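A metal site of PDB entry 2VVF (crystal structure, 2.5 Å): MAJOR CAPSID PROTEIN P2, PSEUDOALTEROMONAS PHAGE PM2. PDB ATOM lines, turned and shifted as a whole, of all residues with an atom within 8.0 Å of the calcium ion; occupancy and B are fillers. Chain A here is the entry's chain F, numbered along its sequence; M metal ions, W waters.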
ATOM      1  N   THR A  28       4.462  24.601   5.217  1.00  0.00           N
ATOM      2  CA  THR A  28       3.739  23.348   5.390  1.00  0.00           C
ATOM      3  C   THR A  28       4.016  22.402   4.228  1.00  0.00           C
ATOM      4  O   THR A  28       3.926  22.796   3.064  1.00  0.00           O
ATOM      5  CB  THR A  28       2.229  23.597   5.544  1.00  0.00           C
ATOM      6  OG1 THR A  28       1.967  24.252   6.786  1.00  0.00           O
ATOM      7  CG2 THR A  28       1.459  22.278   5.504  1.00  0.00           C
ATOM      8  N   TYR A  29       4.336  21.145   4.539  1.00  0.00           N
ATOM      9  CA  TYR A  29       4.595  20.146   3.511  1.00  0.00           C
ATOM     10  C   TYR A  29       3.388  19.245   3.341  1.00  0.00           C
ATOM     11  O   TYR A  29       3.087  18.425   4.221  1.00  0.00           O
ATOM     12  CB  TYR A  29       5.828  19.311   3.877  1.00  0.00           C
ATOM     13  CG  TYR A  29       7.131  20.080   3.844  1.00  0.00           C
ATOM     14  CD1 TYR A  29       7.878  20.188   2.676  1.00  0.00           C
ATOM     15  CD2 TYR A  29       7.609  20.703   4.984  1.00  0.00           C
ATOM     16  CE1 TYR A  29       9.068  20.891   2.654  1.00  0.00           C
ATOM     17  CE2 TYR A  29       8.797  21.405   4.980  1.00  0.00           C
ATOM     18  CZ  TYR A  29       9.520  21.500   3.808  1.00  0.00           C
ATOM     19  OH  TYR A  29      10.702  22.205   3.780  1.00  0.00           O
ATOM     20  N   PHE A  85       1.255  13.513   3.284  1.00  0.00           N
ATOM     21  CA  PHE A  85       0.933  13.987   4.628  1.00  0.00           C
ATOM     22  C   PHE A  85      -0.544  14.373   4.628  1.00  0.00           C
ATOM     23  O   PHE A  85      -1.296  13.975   5.517  1.00  0.00           O
ATOM     24  CB  PHE A  85       1.834  15.164   5.017  1.00  0.00           C
ATOM     25  CG  PHE A  85       3.288  14.787   5.092  1.00  0.00           C
ATOM     26  CD1 PHE A  85       3.742  13.965   6.101  1.00  0.00           C
ATOM     27  CD2 PHE A  85       4.166  15.200   4.106  1.00  0.00           C
ATOM     28  CE1 PHE A  85       5.078  13.589   6.157  1.00  0.00           C
ATOM     29  CE2 PHE A  85       5.502  14.824   4.162  1.00  0.00           C
ATOM     30  CZ  PHE A  85       5.956  14.015   5.190  1.00  0.00           C
ATOM     31  N   VAL A  86      -0.956  15.089   3.586  1.00  0.00           N
ATOM     32  CA  VAL A  86      -2.351  15.442   3.411  1.00  0.00           C
ATOM     33  C   VAL A  86      -3.041  14.175   2.923  1.00  0.00           C
ATOM     34  O   VAL A  86      -2.590  13.536   1.971  1.00  0.00           O
ATOM     35  CB  VAL A  86      -2.507  16.582   2.382  1.00  0.00           C
ATOM     36  CG1 VAL A  86      -3.938  16.631   1.855  1.00  0.00           C
ATOM     37  CG2 VAL A  86      -2.100  17.919   2.989  1.00  0.00           C
ATOM     38  N   GLN A 101      -8.794  16.923   4.782  1.00  0.00           N
ATOM     39  CA  GLN A 101      -7.630  16.336   4.123  1.00  0.00           C
ATOM     40  C   GLN A 101      -6.363  17.123   4.436  1.00  0.00           C
ATOM     41  O   GLN A 101      -5.329  16.549   4.776  1.00  0.00           O
ATOM     42  CB  GLN A 101      -7.840  16.275   2.604  1.00  0.00           C
ATOM     43  CG  GLN A 101      -9.123  15.583   2.186  1.00  0.00           C
ATOM     44  CD  GLN A 101      -9.531  15.937   0.769  1.00  0.00           C
ATOM     45  OE1 GLN A 101      -8.822  16.670   0.067  1.00  0.00           O
ATOM     46  NE2 GLN A 101     -10.673  15.429   0.338  1.00  0.00           N
ATOM     47  N   ARG A 102      -6.450  18.438   4.295  1.00  0.00           N
ATOM     48  CA  ARG A 102      -5.310  19.323   4.537  1.00  0.00           C
ATOM     49  C   ARG A 102      -4.933  19.350   6.013  1.00  0.00           C
ATOM     50  O   ARG A 102      -3.813  19.714   6.373  1.00  0.00           O
ATOM     51  CB  ARG A 102      -5.612  20.742   4.048  1.00  0.00           C
ATOM     52  CG  ARG A 102      -6.025  20.816   2.581  1.00  0.00           C
ATOM     53  CD  ARG A 102      -6.589  22.187   2.245  1.00  0.00           C
ATOM     54  NE  ARG A 102      -6.452  22.504   0.827  1.00  0.00           N
ATOM     55  CZ  ARG A 102      -7.031  23.549   0.234  1.00  0.00           C
ATOM     56  NH1 ARG A 102      -6.844  23.761  -1.058  1.00  0.00           N
ATOM     57  NH2 ARG A 102      -7.790  24.366   0.937  1.00  0.00           N
ATOM     58  N   MET A 103      -5.867  18.943   6.865  1.00  0.00           N
ATOM     59  CA  MET A 103      -5.656  18.911   8.307  1.00  0.00           C
ATOM     60  C   MET A 103      -4.482  18.000   8.684  1.00  0.00           C
ATOM     61  O   MET A 103      -3.942  18.110   9.789  1.00  0.00           O
ATOM     62  CB  MET A 103      -6.936  18.442   9.011  1.00  0.00           C
ATOM     63  CG  MET A 103      -6.830  18.373  10.538  1.00  0.00           C
ATOM     64  SD  MET A 103      -7.615  16.884  11.234  1.00  0.00           S
ATOM     65  CE  MET A 103      -8.616  17.588  12.561  1.00  0.00           C
ATOM     66  N   PHE A 104      -4.096  17.113   7.772  1.00  0.00           N
ATOM     67  CA  PHE A 104      -3.018  16.174   8.026  1.00  0.00           C
ATOM     68  C   PHE A 104      -1.664  16.640   7.481  1.00  0.00           C
ATOM     69  O   PHE A 104      -0.646  15.965   7.673  1.00  0.00           O
ATOM     70  CB  PHE A 104      -3.351  14.787   7.464  1.00  0.00           C
ATOM     71  CG  PHE A 104      -4.452  14.093   8.206  1.00  0.00           C
ATOM     72  CD1 PHE A 104      -4.153  13.247   9.267  1.00  0.00           C
ATOM     73  CD2 PHE A 104      -5.777  14.279   7.852  1.00  0.00           C
ATOM     74  CE1 PHE A 104      -5.159  12.602   9.954  1.00  0.00           C
ATOM     75  CE2 PHE A 104      -6.790  13.635   8.533  1.00  0.00           C
ATOM     76  CZ  PHE A 104      -6.474  12.788   9.589  1.00  0.00           C
ATOM     77  N   ALA A 105      -1.656  17.780   6.796  1.00  0.00           N
ATOM     78  CA  ALA A 105      -0.430  18.319   6.225  1.00  0.00           C
ATOM     79  C   ALA A 105       0.645  18.502   7.294  1.00  0.00           C
ATOM     80  O   ALA A 105       0.349  18.768   8.458  1.00  0.00           O
ATOM     81  CB  ALA A 105      -0.705  19.632   5.521  1.00  0.00           C
ATOM     82  N   LEU A 106       1.909  18.373   6.889  1.00  0.00           N
ATOM     83  CA  LEU A 106       3.035  18.516   7.804  1.00  0.00           C
ATOM     84  C   LEU A 106       3.458  19.968   8.014  1.00  0.00           C
ATOM     85  O   LEU A 106       4.355  20.462   7.339  1.00  0.00           O
ATOM     86  CB  LEU A 106       4.222  17.686   7.327  1.00  0.00           C
ATOM     87  CG  LEU A 106       5.503  17.785   8.151  1.00  0.00           C
ATOM     88  CD1 LEU A 106       5.213  17.486   9.623  1.00  0.00           C
ATOM     89  CD2 LEU A 106       6.562  16.846   7.605  1.00  0.00           C
ATOM     90  N   GLY A 107       2.815  20.638   8.976  1.00  0.00           N
ATOM     91  CA  GLY A 107       3.172  22.014   9.295  1.00  0.00           C
ATOM     92  C   GLY A 107       4.507  21.982  10.040  1.00  0.00           C
ATOM     93  O   GLY A 107       4.775  21.034  10.787  1.00  0.00           O
ATOM     94  N   THR A 108       5.342  22.990   9.827  1.00  0.00           N
ATOM     95  CA  THR A 108       6.650  23.037  10.475  1.00  0.00           C
ATOM     96  C   THR A 108       6.847  24.217  11.421  1.00  0.00           C
ATOM     97  O   THR A 108       7.884  24.329  12.068  1.00  0.00           O
ATOM     98  CB  THR A 108       7.787  22.951   9.430  1.00  0.00           C
ATOM     99  OG1 THR A 108       7.807  24.149   8.634  1.00  0.00           O
ATOM    100  CG2 THR A 108       7.605  21.746   8.524  1.00  0.00           C
ATOM    101  N   THR A 139       2.033  26.220   9.085  1.00  0.00           N
ATOM    102  CA  THR A 139       1.120  25.880  10.165  1.00  0.00           C
ATOM    103  C   THR A 139       1.899  25.034  11.168  1.00  0.00           C
ATOM    104  O   THR A 139       2.953  24.505  10.838  1.00  0.00           O
ATOM    105  CB  THR A 139      -0.106  25.085   9.652  1.00  0.00           C
ATOM    106  OG1 THR A 139       0.304  23.791   9.201  1.00  0.00           O
ATOM    107  CG2 THR A 139      -0.785  25.823   8.507  1.00  0.00           C
ATOM    108  N   ALA A 140       1.381  24.917  12.378  1.00  0.00           N
ATOM    109  CA  ALA A 140       2.025  24.099  13.385  1.00  0.00           C
ATOM    110  C   ALA A 140       1.899  22.651  12.928  1.00  0.00           C
ATOM    111  O   ALA A 140       1.078  22.344  12.070  1.00  0.00           O
ATOM    112  CB  ALA A 140       1.350  24.286  14.739  1.00  0.00           C
ATOM    113  N   PRO A 141       2.735  21.759  13.480  1.00  0.00           N
ATOM    114  CA  PRO A 141       2.663  20.349  13.119  1.00  0.00           C
ATOM    115  C   PRO A 141       1.228  19.863  13.252  1.00  0.00           C
ATOM    116  O   PRO A 141       0.680  19.233  12.342  1.00  0.00           O
ATOM    117  CB  PRO A 141       3.565  19.692  14.161  1.00  0.00           C
ATOM    118  CG  PRO A 141       4.606  20.726  14.462  1.00  0.00           C
ATOM    119  CD  PRO A 141       3.980  22.089  14.194  1.00  0.00           C
ATOM    120  N   SER A 142       0.593  20.215  14.372  1.00  0.00           N
ATOM    121  CA  SER A 142      -0.805  19.873  14.636  1.00  0.00           C
ATOM    122  C   SER A 142      -1.153  18.405  14.398  1.00  0.00           C
ATOM    123  O   SER A 142      -0.352  17.510  14.654  1.00  0.00           O
ATOM    124  CB  SER A 142      -1.732  20.783  13.825  1.00  0.00           C
ATOM    125  OG  SER A 142      -1.542  20.605  12.430  1.00  0.00           O
ATOM    126  N   TRP A 143      -2.373  18.161  13.925  1.00  0.00           N
ATOM    127  CA  TRP A 143      -2.858  16.816  13.664  1.00  0.00           C
ATOM    128  C   TRP A 143      -1.994  16.075  12.639  1.00  0.00           C
ATOM    129  O   TRP A 143      -1.925  16.468  11.476  1.00  0.00           O
ATOM    130  CB  TRP A 143      -4.309  16.863  13.175  1.00  0.00           C
ATOM    131  CG  TRP A 143      -5.003  15.543  13.276  1.00  0.00           C
ATOM    132  CD1 TRP A 143      -5.216  14.654  12.268  1.00  0.00           C
ATOM    133  CD2 TRP A 143      -5.568  14.956  14.459  1.00  0.00           C
ATOM    134  NE1 TRP A 143      -5.863  13.544  12.740  1.00  0.00           N
ATOM    135  CE2 TRP A 143      -6.101  13.707  14.082  1.00  0.00           C
ATOM    136  CE3 TRP A 143      -5.671  15.361  15.787  1.00  0.00           C
ATOM    137  CZ2 TRP A 143      -6.728  12.860  14.994  1.00  0.00           C
ATOM    138  CZ3 TRP A 143      -6.300  14.522  16.687  1.00  0.00           C
ATOM    139  CH2 TRP A 143      -6.821  13.290  16.284  1.00  0.00           C
ATOM    140  N   LEU A 144      -1.348  14.989  13.074  1.00  0.00           N
ATOM    141  CA  LEU A 144      -0.481  14.215  12.194  1.00  0.00           C
ATOM    142  C   LEU A 144      -0.739  12.718  12.260  1.00  0.00           C
ATOM    143  O   LEU A 144      -1.243  12.205  13.262  1.00  0.00           O
ATOM    144  CB  LEU A 144       0.984  14.484  12.544  1.00  0.00           C
ATOM    145  CG  LEU A 144       1.781  15.506  11.721  1.00  0.00           C
ATOM    146  CD1 LEU A 144       0.860  16.530  11.088  1.00  0.00           C
ATOM    147  CD2 LEU A 144       2.817  16.190  12.602  1.00  0.00           C
ATOM    148  N   THR A 145      -0.371  12.008  11.195  1.00  0.00           N
ATOM    149  CA  THR A 145      -0.494  10.562  11.147  1.00  0.00           C
ATOM    150  C   THR A 145       0.822   9.981  11.652  1.00  0.00           C
ATOM    151  O   THR A 145       1.895  10.364  11.186  1.00  0.00           O
ATOM    152  CB  THR A 145      -0.784  10.066   9.704  1.00  0.00           C
ATOM    153  OG1 THR A 145      -2.073  10.518   9.286  1.00  0.00           O
ATOM    154  CG2 THR A 145      -0.744   8.547   9.657  1.00  0.00           C
ATOM    155  N   GLY A 262      -3.099  12.081  15.961  1.00  0.00           N
ATOM    156  CA  GLY A 262      -3.230  12.965  17.099  1.00  0.00           C
ATOM    157  C   GLY A 262      -2.465  14.262  16.870  1.00  0.00           C
ATOM    158  O   GLY A 262      -1.688  14.372  15.927  1.00  0.00           O
ATOM    159  N   VAL A 263      -2.717  15.231  17.734  1.00  0.00           N
ATOM    160  CA  VAL A 263      -2.036  16.521  17.658  1.00  0.00           C
ATOM    161  C   VAL A 263      -0.601  16.320  18.128  1.00  0.00           C
ATOM    162  O   VAL A 263      -0.367  15.933  19.267  1.00  0.00           O
ATOM    163  CB  VAL A 263      -2.748  17.588  18.495  1.00  0.00           C
ATOM    164  CG1 VAL A 263      -1.980  18.897  18.477  1.00  0.00           C
ATOM    165  CG2 VAL A 263      -4.177  17.783  18.003  1.00  0.00           C
ATOM    166  N   TRP A 264       0.352  16.558  17.231  1.00  0.00           N
ATOM    167  CA  TRP A 264       1.757  16.376  17.571  1.00  0.00           C
ATOM    168  C   TRP A 264       2.173  17.218  18.767  1.00  0.00           C
ATOM    169  O   TRP A 264       1.847  18.401  18.863  1.00  0.00           O
ATOM    170  CB  TRP A 264       2.664  16.684  16.371  1.00  0.00           C
ATOM    171  CG  TRP A 264       4.101  16.337  16.621  1.00  0.00           C
ATOM    172  CD1 TRP A 264       4.684  15.115  16.485  1.00  0.00           C
ATOM    173  CD2 TRP A 264       5.128  17.224  17.084  1.00  0.00           C
ATOM    174  NE1 TRP A 264       6.011  15.187  16.812  1.00  0.00           N
ATOM    175  CE2 TRP A 264       6.312  16.469  17.183  1.00  0.00           C
ATOM    176  CE3 TRP A 264       5.161  18.574  17.418  1.00  0.00           C
ATOM    177  CZ2 TRP A 264       7.520  17.023  17.606  1.00  0.00           C
ATOM    178  CZ3 TRP A 264       6.367  19.136  17.831  1.00  0.00           C
ATOM    179  CH2 TRP A 264       7.525  18.355  17.925  1.00  0.00           C
HETATM  180 CA    CA M   1      -1.165  18.902  10.607  1.00  0.00          CA
HETATM  181  O   HOH W   1      -1.063  21.407   9.582  1.00  0.00           O
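The calcium ion is bound by OG of Ser 142, 2.5 Å away.
The calcium ion is bound by O of Pro 141 (2.6 Å).
O of Ala 105 is bound to the calcium ion, 2.6 Å away.
O of Trp 143 binds the calcium ion, at 2.7 Å.
Water W1 binds the calcium ion, at 2.7 Å.
The calcium ion has five donor atoms within binding distance.
Slightly farther from the calcium ion lies O of Met 103 (3.0 Å).
C of Phe 104 touches the calcium ion, 3.9 Å away.
CD1 of Leu 144 touches the calcium ion, 3.2 Å away.
Seven residues have an atom within 4 Å of the calcium ion: Met 103, Phe 104, Ala 105, Pro 141, Ser 142, Trp 143 and Leu 144.
The nearest printed residue that does not touch the calcium ion is Ala 140 (4.4 Å).
The backbone carbonyl oxygen (O) of Ala 140 lies close to the side-chain hydroxyl (OG) of Ser 142, 3.2 Å away.
The backbone carbonyl oxygen (O) of Ser 142 lies within hydrogen-bond range of the backbone NH (N) of Trp 264 (2.8 Å).
N of Leu 144 lies within hydrogen-bond range of O of Gly 262.
Water W1 bridges OG1 of Thr 139 (2.8 Å) and O of Ala 140 (3.4 Å).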
